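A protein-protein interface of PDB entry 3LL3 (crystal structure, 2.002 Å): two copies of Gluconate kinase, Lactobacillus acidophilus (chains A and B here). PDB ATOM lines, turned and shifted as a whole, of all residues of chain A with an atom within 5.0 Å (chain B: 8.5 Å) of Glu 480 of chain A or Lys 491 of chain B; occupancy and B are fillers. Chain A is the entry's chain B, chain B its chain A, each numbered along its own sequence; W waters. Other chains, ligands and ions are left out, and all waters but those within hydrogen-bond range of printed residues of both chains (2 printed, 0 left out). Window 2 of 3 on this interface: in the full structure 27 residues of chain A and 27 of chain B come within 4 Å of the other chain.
Among the printed residues, pairs that only touch across the chains: Leu 477 of chain A with Lys 491 of chain B (3.6 Å), Leu 477 of chain A with Phe 492 of chain B (3.98 Å), Glu 480 of chain A with Lys 491 of chain B (3.4 Å), Ile 481 of chain A with Phe 492 of chain B (3.6 Å), Ala 484 of chain A with Ala 484 of chain B (3.9 Å) and Ala 484 of chain A with Ser 488 of chain B (3.6 Å).
Ala 484 of chain B touches its own counterpart, Ala 484 of chain A. 1 position is printed for both chains. Of the 6 pairs that touch across the chains among the printed residues, 1 has its exchanged pair printed and touching as well.
Hydrophobic or aromatic side chains of chain A within 4 Å of the printed part of chain B: Leu 477, Ile 481 and Ala 484.
Of the printed residues of chain B, Leu 477 of chain A touches Lys 491 (3.6 Å) and Phe 492 (3.98 Å). Glu 480 of chain A touches just one residue of chain B: Lys 491. Printed residues of chain B within 4 Å of Ile 481 of chain A: Phe 492. Printed residues of chain A within 4 Å of Ala 484 of chain B: Ala 484 (3.9 Å). Lys 491 of chain B touches two residues of chain A. Of the printed residues of chain A, Phe 492 of chain B touches Leu 477 and Ile 481. The nearest residue of chain B that does not touch Glu 480 of chain A is Ser 488 of chain B (4.5 Å). The nearest residue of chain A that does not touch Lys 491 of chain B is Pro 476 of chain A (4.5 Å). The nearest printed residue of chain A that does not touch Phe 492 of chain B is Glu 480 of chain A (7.4 Å).
Water W1 bridges OG of Ser 488 of chain B (2.6 Å) and OE1 of Glu 480 of chain A (2.6 Å). Water W2 bridges the backbone carbonyl oxygen of Ala 484 of chain A (2.7 Å) and the backbone carbonyl oxygen of Ala 484 of chain B (2.8 Å).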
ATOM      1  N   PRO A 476     -26.182  -8.358 -12.873  1.00  0.00           N
ATOM      2  CA  PRO A 476     -26.584  -9.544 -12.112  1.00  0.00           C
ATOM      3  C   PRO A 476     -25.762 -10.779 -12.451  1.00  0.00           C
ATOM      4  O   PRO A 476     -25.570 -11.633 -11.589  1.00  0.00           O
ATOM      5  CB  PRO A 476     -28.047  -9.756 -12.538  1.00  0.00           C
ATOM      6  CG  PRO A 476     -28.517  -8.390 -12.883  1.00  0.00           C
ATOM      7  CD  PRO A 476     -27.333  -7.752 -13.570  1.00  0.00           C
ATOM      8  N   LEU A 477     -25.292 -10.884 -13.687  1.00  0.00           N
ATOM      9  CA  LEU A 477     -24.426 -11.985 -14.044  1.00  0.00           C
ATOM     10  C   LEU A 477     -23.066 -11.802 -13.347  1.00  0.00           C
ATOM     11  O   LEU A 477     -22.519 -12.753 -12.789  1.00  0.00           O
ATOM     12  CB  LEU A 477     -24.252 -12.058 -15.557  1.00  0.00           C
ATOM     13  CG  LEU A 477     -23.330 -13.138 -16.124  1.00  0.00           C
ATOM     14  CD1 LEU A 477     -23.747 -14.522 -15.632  1.00  0.00           C
ATOM     15  CD2 LEU A 477     -23.318 -13.071 -17.647  1.00  0.00           C
ATOM     16  N   TYR A 478     -22.533 -10.581 -13.366  1.00  0.00           N
ATOM     17  CA  TYR A 478     -21.282 -10.281 -12.643  1.00  0.00           C
ATOM     18  C   TYR A 478     -21.381 -10.746 -11.169  1.00  0.00           C
ATOM     19  O   TYR A 478     -20.479 -11.414 -10.661  1.00  0.00           O
ATOM     20  CB  TYR A 478     -20.955  -8.780 -12.737  1.00  0.00           C
ATOM     21  CG  TYR A 478     -19.796  -8.303 -11.866  1.00  0.00           C
ATOM     22  CD1 TYR A 478     -18.527  -8.092 -12.405  1.00  0.00           C
ATOM     23  CD2 TYR A 478     -19.984  -8.055 -10.513  1.00  0.00           C
ATOM     24  CE1 TYR A 478     -17.468  -7.654 -11.610  1.00  0.00           C
ATOM     25  CE2 TYR A 478     -18.945  -7.616  -9.718  1.00  0.00           C
ATOM     26  CZ  TYR A 478     -17.687  -7.425 -10.267  1.00  0.00           C
ATOM     27  OH  TYR A 478     -16.682  -6.999  -9.442  1.00  0.00           O
ATOM     28  N   CYS A 479     -22.492 -10.420 -10.506  1.00  0.00           N
ATOM     29  CA  CYS A 479     -22.741 -10.830  -9.110  1.00  0.00           C
ATOM     30  C   CYS A 479     -22.914 -12.349  -8.916  1.00  0.00           C
ATOM     31  O   CYS A 479     -22.504 -12.908  -7.901  1.00  0.00           O
ATOM     32  CB  CYS A 479     -23.988 -10.117  -8.567  1.00  0.00           C
ATOM     33  SG  CYS A 479     -23.812  -8.307  -8.518  1.00  0.00           S
ATOM     34  N   GLU A 480     -23.569 -12.996  -9.870  1.00  0.00           N
ATOM     35  CA  GLU A 480     -23.728 -14.448  -9.835  1.00  0.00           C
ATOM     36  C   GLU A 480     -22.355 -15.126  -9.829  1.00  0.00           C
ATOM     37  O   GLU A 480     -22.114 -16.033  -9.042  1.00  0.00           O
ATOM     38  CB  GLU A 480     -24.555 -14.917 -11.034  1.00  0.00           C
ATOM     39  CG  GLU A 480     -26.020 -15.172 -10.725  1.00  0.00           C
ATOM     40  CD  GLU A 480     -26.377 -16.661 -10.769  1.00  0.00           C
ATOM     41  OE1 GLU A 480     -25.572 -17.451 -11.310  1.00  0.00           O
ATOM     42  OE2 GLU A 480     -27.469 -17.038 -10.277  1.00  0.00           O
ATOM     43  N   ILE A 481     -21.456 -14.658 -10.691  1.00  0.00           N
ATOM     44  CA  ILE A 481     -20.105 -15.213 -10.770  1.00  0.00           C
ATOM     45  C   ILE A 481     -19.273 -14.918  -9.501  1.00  0.00           C
ATOM     46  O   ILE A 481     -18.598 -15.805  -8.965  1.00  0.00           O
ATOM     47  CB  ILE A 481     -19.370 -14.712 -12.030  1.00  0.00           C
ATOM     48  CG1 ILE A 481     -20.187 -15.007 -13.297  1.00  0.00           C
ATOM     49  CG2 ILE A 481     -17.961 -15.316 -12.112  1.00  0.00           C
ATOM     50  CD1 ILE A 481     -20.503 -16.505 -13.541  1.00  0.00           C
ATOM     51  N   ARG A 482     -19.333 -13.673  -9.022  1.00  0.00           N
ATOM     52  CA  ARG A 482     -18.727 -13.308  -7.759  1.00  0.00           C
ATOM     53  C   ARG A 482     -19.203 -14.222  -6.636  1.00  0.00           C
ATOM     54  O   ARG A 482     -18.390 -14.738  -5.855  1.00  0.00           O
ATOM     55  CB  ARG A 482     -19.030 -11.835  -7.421  1.00  0.00           C
ATOM     56  CG  ARG A 482     -18.750 -11.427  -5.953  1.00  0.00           C
ATOM     57  CD  ARG A 482     -20.083 -11.212  -5.195  1.00  0.00           C
ATOM     58  NE  ARG A 482     -20.590  -9.871  -5.430  1.00  0.00           N
ATOM     59  CZ  ARG A 482     -21.846  -9.453  -5.257  1.00  0.00           C
ATOM     60  NH1 ARG A 482     -22.820 -10.270  -4.853  1.00  0.00           N
ATOM     61  NH2 ARG A 482     -22.125  -8.181  -5.510  1.00  0.00           N
ATOM     62  N   ASN A 483     -20.521 -14.394  -6.547  1.00  0.00           N
ATOM     63  CA  ASN A 483     -21.139 -15.261  -5.541  1.00  0.00           C
ATOM     64  C   ASN A 483     -20.692 -16.725  -5.666  1.00  0.00           C
ATOM     65  O   ASN A 483     -20.454 -17.402  -4.665  1.00  0.00           O
ATOM     66  CB  ASN A 483     -22.675 -15.208  -5.650  1.00  0.00           C
ATOM     67  CG  ASN A 483     -23.262 -13.862  -5.225  1.00  0.00           C
ATOM     68  OD1 ASN A 483     -22.600 -13.047  -4.586  1.00  0.00           O
ATOM     69  ND2 ASN A 483     -24.525 -13.635  -5.585  1.00  0.00           N
ATOM     70  N   ALA A 484     -20.605 -17.208  -6.904  1.00  0.00           N
ATOM     71  CA  ALA A 484     -20.219 -18.591  -7.163  1.00  0.00           C
ATOM     72  C   ALA A 484     -18.816 -18.876  -6.640  1.00  0.00           C
ATOM     73  O   ALA A 484     -18.544 -19.948  -6.120  1.00  0.00           O
ATOM     74  CB  ALA A 484     -20.286 -18.880  -8.664  1.00  0.00           C
ATOM     75  N   ASN B 351     -23.381 -26.091 -22.507  1.00  0.00           N
ATOM     76  CA  ASN B 351     -23.395 -24.647 -22.273  1.00  0.00           C
ATOM     77  C   ASN B 351     -22.161 -24.137 -21.557  1.00  0.00           C
ATOM     78  O   ASN B 351     -22.003 -22.935 -21.369  1.00  0.00           O
ATOM     79  CB  ASN B 351     -24.653 -24.232 -21.506  1.00  0.00           C
ATOM     80  CG  ASN B 351     -25.904 -24.671 -22.202  1.00  0.00           C
ATOM     81  OD1 ASN B 351     -26.036 -24.508 -23.416  1.00  0.00           O
ATOM     82  ND2 ASN B 351     -26.819 -25.269 -21.452  1.00  0.00           N
ATOM     83  N   ARG B 353     -18.505 -22.831 -20.441  1.00  0.00           N
ATOM     84  CA  ARG B 353     -17.598 -21.874 -21.046  1.00  0.00           C
ATOM     85  C   ARG B 353     -16.261 -21.924 -20.299  1.00  0.00           C
ATOM     86  O   ARG B 353     -16.170 -22.540 -19.251  1.00  0.00           O
ATOM     87  CB  ARG B 353     -18.215 -20.477 -21.021  1.00  0.00           C
ATOM     88  CG  ARG B 353     -19.366 -20.320 -22.018  1.00  0.00           C
ATOM     89  CD  ARG B 353     -20.143 -19.062 -21.722  1.00  0.00           C
ATOM     90  NE  ARG B 353     -20.444 -18.314 -22.936  1.00  0.00           N
ATOM     91  CZ  ARG B 353     -21.620 -18.327 -23.547  1.00  0.00           C
ATOM     92  NH1 ARG B 353     -22.612 -19.051 -23.051  1.00  0.00           N
ATOM     93  NH2 ARG B 353     -21.805 -17.617 -24.649  1.00  0.00           N
ATOM     94  N   ALA B 484     -17.160 -25.333  -8.429  1.00  0.00           N
ATOM     95  CA  ALA B 484     -17.745 -24.073  -7.955  1.00  0.00           C
ATOM     96  C   ALA B 484     -18.557 -23.414  -9.056  1.00  0.00           C
ATOM     97  O   ALA B 484     -19.583 -22.791  -8.801  1.00  0.00           O
ATOM     98  CB  ALA B 484     -16.661 -23.126  -7.456  1.00  0.00           C
ATOM     99  N   LEU B 485     -18.098 -23.578 -10.291  1.00  0.00           N
ATOM    100  CA  LEU B 485     -18.718 -22.930 -11.442  1.00  0.00           C
ATOM    101  C   LEU B 485     -19.683 -23.823 -12.225  1.00  0.00           C
ATOM    102  O   LEU B 485     -20.358 -23.341 -13.120  1.00  0.00           O
ATOM    103  CB  LEU B 485     -17.641 -22.378 -12.391  1.00  0.00           C
ATOM    104  CG  LEU B 485     -16.874 -21.161 -11.848  1.00  0.00           C
ATOM    105  CD1 LEU B 485     -15.661 -20.880 -12.707  1.00  0.00           C
ATOM    106  CD2 LEU B 485     -17.810 -19.945 -11.787  1.00  0.00           C
ATOM    107  N   ALA B 486     -19.732 -25.111 -11.904  1.00  0.00           N
ATOM    108  CA  ALA B 486     -20.512 -26.069 -12.702  1.00  0.00           C
ATOM    109  C   ALA B 486     -21.967 -25.629 -12.940  1.00  0.00           C
ATOM    110  O   ALA B 486     -22.497 -25.778 -14.032  1.00  0.00           O
ATOM    111  CB  ALA B 486     -20.463 -27.462 -12.076  1.00  0.00           C
ATOM    112  N   ALA B 487     -22.606 -25.056 -11.931  1.00  0.00           N
ATOM    113  CA  ALA B 487     -24.004 -24.664 -12.083  1.00  0.00           C
ATOM    114  C   ALA B 487     -24.201 -23.234 -12.610  1.00  0.00           C
ATOM    115  O   ALA B 487     -25.323 -22.738 -12.653  1.00  0.00           O
ATOM    116  CB  ALA B 487     -24.767 -24.866 -10.768  1.00  0.00           C
ATOM    117  N   SER B 488     -23.126 -22.581 -13.042  1.00  0.00           N
ATOM    118  CA  SER B 488     -23.225 -21.164 -13.387  1.00  0.00           C
ATOM    119  C   SER B 488     -23.265 -20.827 -14.884  1.00  0.00           C
ATOM    120  O   SER B 488     -23.381 -19.659 -15.250  1.00  0.00           O
ATOM    121  CB  SER B 488     -22.111 -20.370 -12.681  1.00  0.00           C
ATOM    122  OG  SER B 488     -22.250 -20.458 -11.266  1.00  0.00           O
ATOM    123  N   TYR B 489     -23.197 -21.839 -15.746  1.00  0.00           N
ATOM    124  CA  TYR B 489     -23.024 -21.592 -17.177  1.00  0.00           C
ATOM    125  C   TYR B 489     -24.315 -21.205 -17.918  1.00  0.00           C
ATOM    126  O   TYR B 489     -24.270 -20.491 -18.924  1.00  0.00           O
ATOM    127  CB  TYR B 489     -22.320 -22.776 -17.852  1.00  0.00           C
ATOM    128  CG  TYR B 489     -20.954 -23.070 -17.270  1.00  0.00           C
ATOM    129  CD1 TYR B 489     -20.626 -24.347 -16.831  1.00  0.00           C
ATOM    130  CD2 TYR B 489     -20.003 -22.053 -17.121  1.00  0.00           C
ATOM    131  CE1 TYR B 489     -19.381 -24.622 -16.292  1.00  0.00           C
ATOM    132  CE2 TYR B 489     -18.740 -22.319 -16.578  1.00  0.00           C
ATOM    133  CZ  TYR B 489     -18.441 -23.606 -16.168  1.00  0.00           C
ATOM    134  OH  TYR B 489     -17.218 -23.879 -15.619  1.00  0.00           O
ATOM    135  N   GLY B 490     -25.460 -21.653 -17.407  1.00  0.00           N
ATOM    136  CA  GLY B 490     -26.729 -21.425 -18.085  1.00  0.00           C
ATOM    137  C   GLY B 490     -27.017 -19.941 -18.142  1.00  0.00           C
ATOM    138  O   GLY B 490     -27.657 -19.432 -19.059  1.00  0.00           O
ATOM    139  N   LYS B 491     -26.497 -19.254 -17.139  1.00  0.00           N
ATOM    140  CA  LYS B 491     -26.630 -17.818 -16.978  1.00  0.00           C
ATOM    141  C   LYS B 491     -26.114 -17.038 -18.201  1.00  0.00           C
ATOM    142  O   LYS B 491     -26.713 -16.042 -18.596  1.00  0.00           O
ATOM    143  CB  LYS B 491     -25.861 -17.420 -15.712  1.00  0.00           C
ATOM    144  CG  LYS B 491     -26.596 -16.488 -14.757  1.00  0.00           C
ATOM    145  CD  LYS B 491     -28.027 -16.955 -14.484  1.00  0.00           C
ATOM    146  CE  LYS B 491     -28.664 -16.133 -13.362  1.00  0.00           C
ATOM    147  NZ  LYS B 491     -28.305 -14.681 -13.457  1.00  0.00           N
ATOM    148  N   PHE B 492     -25.016 -17.499 -18.804  1.00  0.00           N
ATOM    149  CA  PHE B 492     -24.370 -16.783 -19.911  1.00  0.00           C
ATOM    150  C   PHE B 492     -25.201 -16.699 -21.188  1.00  0.00           C
ATOM    151  O   PHE B 492     -24.746 -16.152 -22.200  1.00  0.00           O
ATOM    152  CB  PHE B 492     -22.990 -17.391 -20.222  1.00  0.00           C
ATOM    153  CG  PHE B 492     -21.971 -17.110 -19.162  1.00  0.00           C
ATOM    154  CD1 PHE B 492     -21.884 -17.915 -18.039  1.00  0.00           C
ATOM    155  CD2 PHE B 492     -21.141 -15.994 -19.253  1.00  0.00           C
ATOM    156  CE1 PHE B 492     -20.954 -17.631 -17.029  1.00  0.00           C
ATOM    157  CE2 PHE B 492     -20.216 -15.704 -18.250  1.00  0.00           C
ATOM    158  CZ  PHE B 492     -20.128 -16.519 -17.137  1.00  0.00           C
ATOM    159  N   SER B 493     -26.420 -17.223 -21.144  1.00  0.00           N
ATOM    160  CA  SER B 493     -27.226 -17.307 -22.354  1.00  0.00           C
ATOM    161  C   SER B 493     -28.661 -17.760 -22.069  1.00  0.00           C
ATOM    162  O   SER B 493     -29.252 -17.395 -21.048  1.00  0.00           O
ATOM    163  CB  SER B 493     -26.546 -18.256 -23.346  1.00  0.00           C
ATOM    164  OG  SER B 493     -27.218 -18.261 -24.590  1.00  0.00           O
HETATM  165  O   HOH W   1     -24.345 -19.471 -10.162  1.00  0.00           O
HETATM  166  O   HOH W   2     -20.197 -22.066  -6.203  1.00  0.00           O
